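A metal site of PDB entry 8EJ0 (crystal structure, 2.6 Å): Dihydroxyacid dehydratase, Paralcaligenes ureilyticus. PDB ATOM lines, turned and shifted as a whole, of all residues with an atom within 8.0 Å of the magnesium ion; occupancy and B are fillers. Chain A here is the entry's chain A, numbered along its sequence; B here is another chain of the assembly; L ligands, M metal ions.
The side-chain carboxylate (OD2) of Asp 126 binds the magnesium ion.
The magnesium ion is bound by OQ1 of KCX 127 (2.2 Å).
The magnesium ion is bound by OE2 of Glu 449, at 2.2 Å.
O2 of LIG L1 binds the magnesium ion (2.2 Å).
OE2 of Glu 89 is bound to the magnesium ion, 2.2 Å away.
O1 of LIG L1 is bound to the magnesium ion, 2.5 Å away.
The magnesium ion has six donor atoms within binding distance.
OQ2 of KCX 127 sits at hydrogen-bond distance from the side-chain hydroxyl (OG1) of Thr 203.
The guanidinium group (NH1) of Arg 474 sits close to the side-chain carboxylate (OE2) of Glu 449, at 3.2 Å.
The side-chain carboxylate (OD1) of Asp 126 sits at hydrogen-bond distance from the backbone NH (N) of Ala 204.
NE2 of His 575 of chain B lies within hydrogen-bond range of OE1 of Glu 449, 2.9 Å away.
The side-chain amide nitrogen (ND2) of Asn 574 of chain B is in hydrogen-bond range of the backbone carbonyl oxygen (O) of Glu 89 (3.4 Å).
The side-chain carboxylate of Glu 449 lies close to the side-chain amide nitrogen of Asn 276 (3.3 Å).
OQ2 of KCX 127 is in hydrogen-bond range of the side-chain amide nitrogen (ND2) of Asn 276, 2.7 Å away.
OQ2 of KCX 127 lies within salt-bridge range of the guanidinium group of Arg 474 (3.5 Å).
Merely in contact with the magnesium ion: Thr 203.
Five residues have an atom within 4 Å of the magnesium ion: Glu 89, Asp 126, KCX 127, Thr 203 and Glu 449.
The nearest printed residue that does not touch the magnesium ion is Asn 276 (4.1 Å).
SG of Cys 125 binds FE1 of LG2 L2 (2.4 Å).
The side-chain sulfur (SG) of Cys 198 binds an iron atom (FE2) of LG2 L2, 2.5 Å away.
N of Cys 198 lies close to S1 of LG2 L2, 3.6 Å away.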
ATOM      1  N   GLY A  88      22.840 -28.563   9.091  1.00  0.00           N
ATOM      2  CA  GLY A  88      21.446 -28.443   9.458  1.00  0.00           C
ATOM      3  C   GLY A  88      21.013 -27.001   9.539  1.00  0.00           C
ATOM      4  O   GLY A  88      21.606 -26.216  10.286  1.00  0.00           O
ATOM      5  N   GLU A  89      19.977 -26.628   8.766  1.00  0.00           N
ATOM      6  CA  GLU A  89      19.496 -25.250   8.738  1.00  0.00           C
ATOM      7  C   GLU A  89      19.187 -24.742  10.134  1.00  0.00           C
ATOM      8  O   GLU A  89      19.762 -23.754  10.597  1.00  0.00           O
ATOM      9  CB  GLU A  89      18.236 -25.154   7.870  1.00  0.00           C
ATOM     10  CG  GLU A  89      18.496 -25.040   6.391  1.00  0.00           C
ATOM     11  CD  GLU A  89      19.332 -23.824   6.051  1.00  0.00           C
ATOM     12  OE1 GLU A  89      20.552 -23.981   5.862  1.00  0.00           O
ATOM     13  OE2 GLU A  89      18.772 -22.704   5.986  1.00  0.00           O
ATOM     14  N   THR A  90      18.253 -25.409  10.820  1.00  0.00           N
ATOM     15  CA  THR A  90      17.759 -24.924  12.097  1.00  0.00           C
ATOM     16  C   THR A  90      18.815 -24.957  13.196  1.00  0.00           C
ATOM     17  O   THR A  90      18.665 -24.271  14.202  1.00  0.00           O
ATOM     18  CB  THR A  90      16.540 -25.747  12.520  1.00  0.00           C
ATOM     19  OG1 THR A  90      16.930 -27.106  12.740  1.00  0.00           O
ATOM     20  CG2 THR A  90      15.473 -25.698  11.431  1.00  0.00           C
ATOM     21  N   THR A  95      24.358 -18.973  10.651  1.00  0.00           N
ATOM     22  CA  THR A  95      23.565 -19.499   9.548  1.00  0.00           C
ATOM     23  C   THR A  95      24.367 -20.603   8.869  1.00  0.00           C
ATOM     24  O   THR A  95      25.589 -20.587   8.892  1.00  0.00           O
ATOM     25  CB  THR A  95      23.172 -18.414   8.533  1.00  0.00           C
ATOM     26  OG1 THR A  95      22.332 -18.989   7.514  1.00  0.00           O
ATOM     27  CG2 THR A  95      24.409 -17.801   7.893  1.00  0.00           C
ATOM     28  N   ALA A  96      23.645 -21.554   8.262  1.00  0.00           N
ATOM     29  CA  ALA A  96      24.315 -22.676   7.622  1.00  0.00           C
ATOM     30  C   ALA A  96      25.055 -22.269   6.364  1.00  0.00           C
ATOM     31  O   ALA A  96      25.986 -22.967   5.945  1.00  0.00           O
ATOM     32  CB  ALA A  96      23.311 -23.785   7.316  1.00  0.00           C
ATOM     33  N   MET A  97      24.665 -21.150   5.744  1.00  0.00           N
ATOM     34  CA  MET A  97      25.396 -20.669   4.568  1.00  0.00           C
ATOM     35  C   MET A  97      26.828 -20.302   4.918  1.00  0.00           C
ATOM     36  O   MET A  97      27.717 -20.360   4.047  1.00  0.00           O
ATOM     37  CB  MET A  97      24.662 -19.468   3.964  1.00  0.00           C
ATOM     38  CG  MET A  97      25.407 -18.769   2.833  1.00  0.00           C
ATOM     39  SD  MET A  97      25.589 -19.771   1.351  1.00  0.00           S
ATOM     40  CE  MET A  97      24.075 -19.377   0.483  1.00  0.00           C
ATOM     41  N   CYS A 125      19.141 -31.654   3.497  1.00  0.00           N
ATOM     42  CA  CYS A 125      18.926 -30.383   4.186  1.00  0.00           C
ATOM     43  C   CYS A 125      19.568 -29.240   3.407  1.00  0.00           C
ATOM     44  O   CYS A 125      20.790 -29.203   3.250  1.00  0.00           O
ATOM     45  CB  CYS A 125      19.505 -30.461   5.603  1.00  0.00           C
ATOM     46  SG  CYS A 125      18.859 -29.242   6.764  1.00  0.00           S
ATOM     47  N   ASP A 126      18.719 -28.324   2.945  1.00  0.00           N
ATOM     48  CA  ASP A 126      19.088 -27.106   2.191  1.00  0.00           C
ATOM     49  C   ASP A 126      20.519 -27.046   1.653  1.00  0.00           C
ATOM     50  O   ASP A 126      20.771 -27.404   0.500  1.00  0.00           O
ATOM     51  CB  ASP A 126      18.864 -25.876   3.061  1.00  0.00           C
ATOM     52  CG  ASP A 126      17.399 -25.513   3.205  1.00  0.00           C
ATOM     53  OD1 ASP A 126      16.544 -26.291   2.722  1.00  0.00           O
ATOM     54  OD2 ASP A 126      17.110 -24.450   3.793  1.00  0.00           O
ATOM     55  N   KCX A 127      21.431 -26.598   2.503  1.00  0.00           N
ATOM     56  CA  KCX A 127      22.797 -26.310   2.092  1.00  0.00           C
ATOM     57  CB  KCX A 127      23.505 -25.502   3.193  1.00  0.00           C
ATOM     58  CG  KCX A 127      23.624 -24.029   2.829  1.00  0.00           C
ATOM     59  CD  KCX A 127      22.759 -23.150   3.721  1.00  0.00           C
ATOM     60  CE  KCX A 127      22.255 -21.910   2.998  1.00  0.00           C
ATOM     61  NZ  KCX A 127      21.283 -22.268   1.983  1.00  0.00           N
ATOM     62  C   KCX A 127      23.619 -27.554   1.781  1.00  0.00           C
ATOM     63  O   KCX A 127      24.639 -27.437   1.187  1.00  0.00           O
ATOM     64  CX  KCX A 127      19.865 -22.213   2.278  1.00  0.00           C
ATOM     65  OQ1 KCX A 127      19.475 -22.268   3.476  1.00  0.00           O
ATOM     66  OQ2 KCX A 127      19.031 -22.099   1.355  1.00  0.00           O
ATOM     67  N   TRP A 168       6.477 -18.771   9.806  1.00  0.00           N
ATOM     68  CA  TRP A 168       6.364 -17.334   9.628  1.00  0.00           C
ATOM     69  C   TRP A 168       4.919 -16.874   9.811  1.00  0.00           C
ATOM     70  O   TRP A 168       4.658 -15.811  10.381  1.00  0.00           O
ATOM     71  CB  TRP A 168       6.875 -16.911   8.252  1.00  0.00           C
ATOM     72  CG  TRP A 168       8.070 -17.670   7.751  1.00  0.00           C
ATOM     73  CD1 TRP A 168       8.144 -18.405   6.606  1.00  0.00           C
ATOM     74  CD2 TRP A 168       9.355 -17.771   8.377  1.00  0.00           C
ATOM     75  NE1 TRP A 168       9.395 -18.961   6.487  1.00  0.00           N
ATOM     76  CE2 TRP A 168      10.157 -18.583   7.554  1.00  0.00           C
ATOM     77  CE3 TRP A 168       9.906 -17.252   9.558  1.00  0.00           C
ATOM     78  CZ2 TRP A 168      11.483 -18.897   7.870  1.00  0.00           C
ATOM     79  CZ3 TRP A 168      11.225 -17.559   9.866  1.00  0.00           C
ATOM     80  CH2 TRP A 168      11.991 -18.371   9.025  1.00  0.00           C
ATOM     81  N   CYS A 198      12.182 -30.211   4.603  1.00  0.00           N
ATOM     82  CA  CYS A 198      10.984 -29.375   4.627  1.00  0.00           C
ATOM     83  C   CYS A 198       9.993 -29.776   3.546  1.00  0.00           C
ATOM     84  O   CYS A 198      10.356 -29.919   2.381  1.00  0.00           O
ATOM     85  CB  CYS A 198      11.390 -27.907   4.469  1.00  0.00           C
ATOM     86  SG  CYS A 198      12.547 -27.333   5.718  1.00  0.00           S
ATOM     87  N   GLY A 202      10.447 -25.144  -0.081  1.00  0.00           N
ATOM     88  CA  GLY A 202      11.593 -24.435   0.432  1.00  0.00           C
ATOM     89  C   GLY A 202      12.828 -24.740  -0.401  1.00  0.00           C
ATOM     90  O   GLY A 202      12.738 -25.245  -1.519  1.00  0.00           O
ATOM     91  N   THR A 203      13.989 -24.441   0.174  1.00  0.00           N
ATOM     92  CA  THR A 203      15.227 -24.648  -0.565  1.00  0.00           C
ATOM     93  C   THR A 203      15.490 -26.133  -0.812  1.00  0.00           C
ATOM     94  O   THR A 203      15.892 -26.512  -1.924  1.00  0.00           O
ATOM     95  CB  THR A 203      16.403 -24.021   0.182  1.00  0.00           C
ATOM     96  OG1 THR A 203      16.116 -22.639   0.460  1.00  0.00           O
ATOM     97  CG2 THR A 203      17.672 -24.099  -0.664  1.00  0.00           C
ATOM     98  N   ALA A 204      15.265 -26.974   0.187  1.00  0.00           N
ATOM     99  CA  ALA A 204      15.531 -28.402   0.041  1.00  0.00           C
ATOM    100  C   ALA A 204      14.699 -29.015  -1.080  1.00  0.00           C
ATOM    101  O   ALA A 204      15.231 -29.714  -1.951  1.00  0.00           O
ATOM    102  CB  ALA A 204      15.284 -29.126   1.356  1.00  0.00           C
ATOM    103  N   SER A 274      12.682 -21.770  -4.613  1.00  0.00           N
ATOM    104  CA  SER A 274      13.249 -20.861  -3.625  1.00  0.00           C
ATOM    105  C   SER A 274      14.223 -19.878  -4.281  1.00  0.00           C
ATOM    106  O   SER A 274      14.835 -20.166  -5.316  1.00  0.00           O
ATOM    107  CB  SER A 274      13.976 -21.653  -2.542  1.00  0.00           C
ATOM    108  OG  SER A 274      14.766 -20.801  -1.730  1.00  0.00           O
ATOM    109  N   ASN A 276      16.972 -19.045  -2.914  1.00  0.00           N
ATOM    110  CA  ASN A 276      18.317 -19.514  -2.630  1.00  0.00           C
ATOM    111  C   ASN A 276      18.894 -20.333  -3.782  1.00  0.00           C
ATOM    112  O   ASN A 276      20.115 -20.413  -3.937  1.00  0.00           O
ATOM    113  CB  ASN A 276      18.332 -20.332  -1.340  1.00  0.00           C
ATOM    114  CG  ASN A 276      18.052 -19.492  -0.113  1.00  0.00           C
ATOM    115  OD1 ASN A 276      18.474 -18.338  -0.032  1.00  0.00           O
ATOM    116  ND2 ASN A 276      17.334 -20.062   0.850  1.00  0.00           N
ATOM    117  N   HIS A 280      22.815 -20.729  -5.341  1.00  0.00           N
ATOM    118  CA  HIS A 280      23.498 -22.021  -5.340  1.00  0.00           C
ATOM    119  C   HIS A 280      23.828 -22.485  -6.753  1.00  0.00           C
ATOM    120  O   HIS A 280      24.914 -23.034  -6.987  1.00  0.00           O
ATOM    121  CB  HIS A 280      22.643 -23.053  -4.616  1.00  0.00           C
ATOM    122  CG  HIS A 280      22.443 -22.756  -3.163  1.00  0.00           C
ATOM    123  ND1 HIS A 280      23.490 -22.438  -2.317  1.00  0.00           N
ATOM    124  CD2 HIS A 280      21.320 -22.719  -2.397  1.00  0.00           C
ATOM    125  CE1 HIS A 280      23.027 -22.228  -1.102  1.00  0.00           C
ATOM    126  NE2 HIS A 280      21.706 -22.388  -1.123  1.00  0.00           N
ATOM    127  N   GLU A 449      19.088 -15.841   6.655  1.00  0.00           N
ATOM    128  CA  GLU A 449      17.738 -15.728   6.094  1.00  0.00           C
ATOM    129  C   GLU A 449      16.920 -14.779   6.963  1.00  0.00           C
ATOM    130  O   GLU A 449      16.035 -15.170   7.722  1.00  0.00           O
ATOM    131  CB  GLU A 449      17.094 -17.107   6.005  1.00  0.00           C
ATOM    132  CG  GLU A 449      17.868 -18.094   5.132  1.00  0.00           C
ATOM    133  CD  GLU A 449      17.236 -19.472   5.109  1.00  0.00           C
ATOM    134  OE1 GLU A 449      16.490 -19.798   6.054  1.00  0.00           O
ATOM    135  OE2 GLU A 449      17.499 -20.225   4.149  1.00  0.00           O
ATOM    136  N   ARG A 474      19.611 -13.090   2.700  1.00  0.00           N
ATOM    137  CA  ARG A 474      18.840 -14.128   2.039  1.00  0.00           C
ATOM    138  C   ARG A 474      17.476 -14.262   2.699  1.00  0.00           C
ATOM    139  O   ARG A 474      17.096 -13.487   3.577  1.00  0.00           O
ATOM    140  CB  ARG A 474      19.590 -15.456   2.059  1.00  0.00           C
ATOM    141  CG  ARG A 474      20.727 -15.567   1.061  1.00  0.00           C
ATOM    142  CD  ARG A 474      21.350 -16.958   1.089  1.00  0.00           C
ATOM    143  NE  ARG A 474      21.653 -17.412   2.444  1.00  0.00           N
ATOM    144  CZ  ARG A 474      20.946 -18.318   3.106  1.00  0.00           C
ATOM    145  NH1 ARG A 474      19.895 -18.882   2.531  1.00  0.00           N
ATOM    146  NH2 ARG A 474      21.288 -18.674   4.332  1.00  0.00           N
ATOM    147  N   MET A 475      16.732 -15.283   2.276  1.00  0.00           N
ATOM    148  CA  MET A 475      15.419 -15.570   2.831  1.00  0.00           C
ATOM    149  C   MET A 475      15.178 -17.065   2.721  1.00  0.00           C
ATOM    150  O   MET A 475      15.592 -17.697   1.745  1.00  0.00           O
ATOM    151  CB  MET A 475      14.325 -14.787   2.100  1.00  0.00           C
ATOM    152  CG  MET A 475      12.968 -15.441   2.152  1.00  0.00           C
ATOM    153  SD  MET A 475      11.751 -14.659   1.092  1.00  0.00           S
ATOM    154  CE  MET A 475      11.800 -13.013   1.777  1.00  0.00           C
ATOM    155  N   SER A 476      14.522 -17.627   3.734  1.00  0.00           N
ATOM    156  CA  SER A 476      14.127 -19.035   3.675  1.00  0.00           C
ATOM    157  C   SER A 476      13.242 -19.279   2.452  1.00  0.00           C
ATOM    158  O   SER A 476      12.357 -18.497   2.137  1.00  0.00           O
ATOM    159  CB  SER A 476      13.385 -19.425   4.950  1.00  0.00           C
ATOM    160  OG  SER A 476      12.819 -20.721   4.830  1.00  0.00           O
ATOM    161  N   GLY A 477      13.500 -20.395   1.765  1.00  0.00           N
ATOM    162  CA  GLY A 477      12.677 -20.767   0.629  1.00  0.00           C
ATOM    163  C   GLY A 477      11.220 -20.975   0.981  1.00  0.00           C
ATOM    164  O   GLY A 477      10.372 -20.981   0.078  1.00  0.00           O
ATOM    165  N   THR A 478      10.922 -21.146   2.258  1.00  0.00           N
ATOM    166  CA  THR A 478       9.557 -21.299   2.744  1.00  0.00           C
ATOM    167  C   THR A 478       8.872 -19.968   3.030  1.00  0.00           C
ATOM    168  O   THR A 478       7.694 -19.963   3.386  1.00  0.00           O
ATOM    169  CB  THR A 478       9.549 -22.156   4.005  1.00  0.00           C
ATOM    170  OG1 THR A 478      10.074 -21.396   5.101  1.00  0.00           O
ATOM    171  CG2 THR A 478      10.416 -23.396   3.815  1.00  0.00           C
ATOM    172  N   ASN B 574      19.715 -17.668  13.336  1.00  0.00           N
ATOM    173  CA  ASN B 574      19.792 -17.937  11.905  1.00  0.00           C
ATOM    174  C   ASN B 574      18.628 -17.356  11.116  1.00  0.00           C
ATOM    175  O   ASN B 574      18.567 -17.548   9.895  1.00  0.00           O
ATOM    176  CB  ASN B 574      19.898 -19.443  11.649  1.00  0.00           C
ATOM    177  CG  ASN B 574      19.034 -20.255  12.593  1.00  0.00           C
ATOM    178  OD1 ASN B 574      17.929 -19.850  12.954  1.00  0.00           O
ATOM    179  ND2 ASN B 574      19.545 -21.416  13.001  1.00  0.00           N
ATOM    180  N   HIS B 575      17.705 -16.661  11.769  1.00  0.00           N
ATOM    181  CA  HIS B 575      16.597 -16.011  11.077  1.00  0.00           C
ATOM    182  C   HIS B 575      16.215 -14.705  11.761  1.00  0.00           C
ATOM    183  O   HIS B 575      16.668 -14.415  12.860  1.00  0.00           O
ATOM    184  CB  HIS B 575      15.381 -16.946  11.011  1.00  0.00           C
ATOM    185  CG  HIS B 575      15.643 -18.218  10.279  1.00  0.00           C
ATOM    186  ND1 HIS B 575      16.185 -19.325  10.883  1.00  0.00           N
ATOM    187  CD2 HIS B 575      15.433 -18.565   8.979  1.00  0.00           C
ATOM    188  CE1 HIS B 575      16.303 -20.307   9.996  1.00  0.00           C
ATOM    189  NE2 HIS B 575      15.859 -19.867   8.837  1.00  0.00           N
HETATM  190  C1  LIG L   1      14.888 -22.753   3.600  1.00  0.00           C
HETATM  191  O1  LIG L   1      15.038 -22.683   4.970  1.00  0.00           O
HETATM  192  O2  LIG L   1      15.724 -22.222   2.882  1.00  0.00           O
HETATM  193  O3  LIG L   1      13.958 -23.613   3.064  1.00  0.00           O
HETATM  194 FE1  LG2 L   2      16.507 -28.854   6.520  1.00  0.00          FE
HETATM  195 FE2  LG2 L   2      14.859 -26.448   5.718  1.00  0.00          FE
HETATM  196  S1  LG2 L   2      15.272 -28.381   4.769  1.00  0.00           S
HETATM  197  S2  LG2 L   2      15.455 -27.288   7.654  1.00  0.00           S
HETATM  198 MG    MG M   1      17.439 -22.398   4.207  1.00  0.00          MG
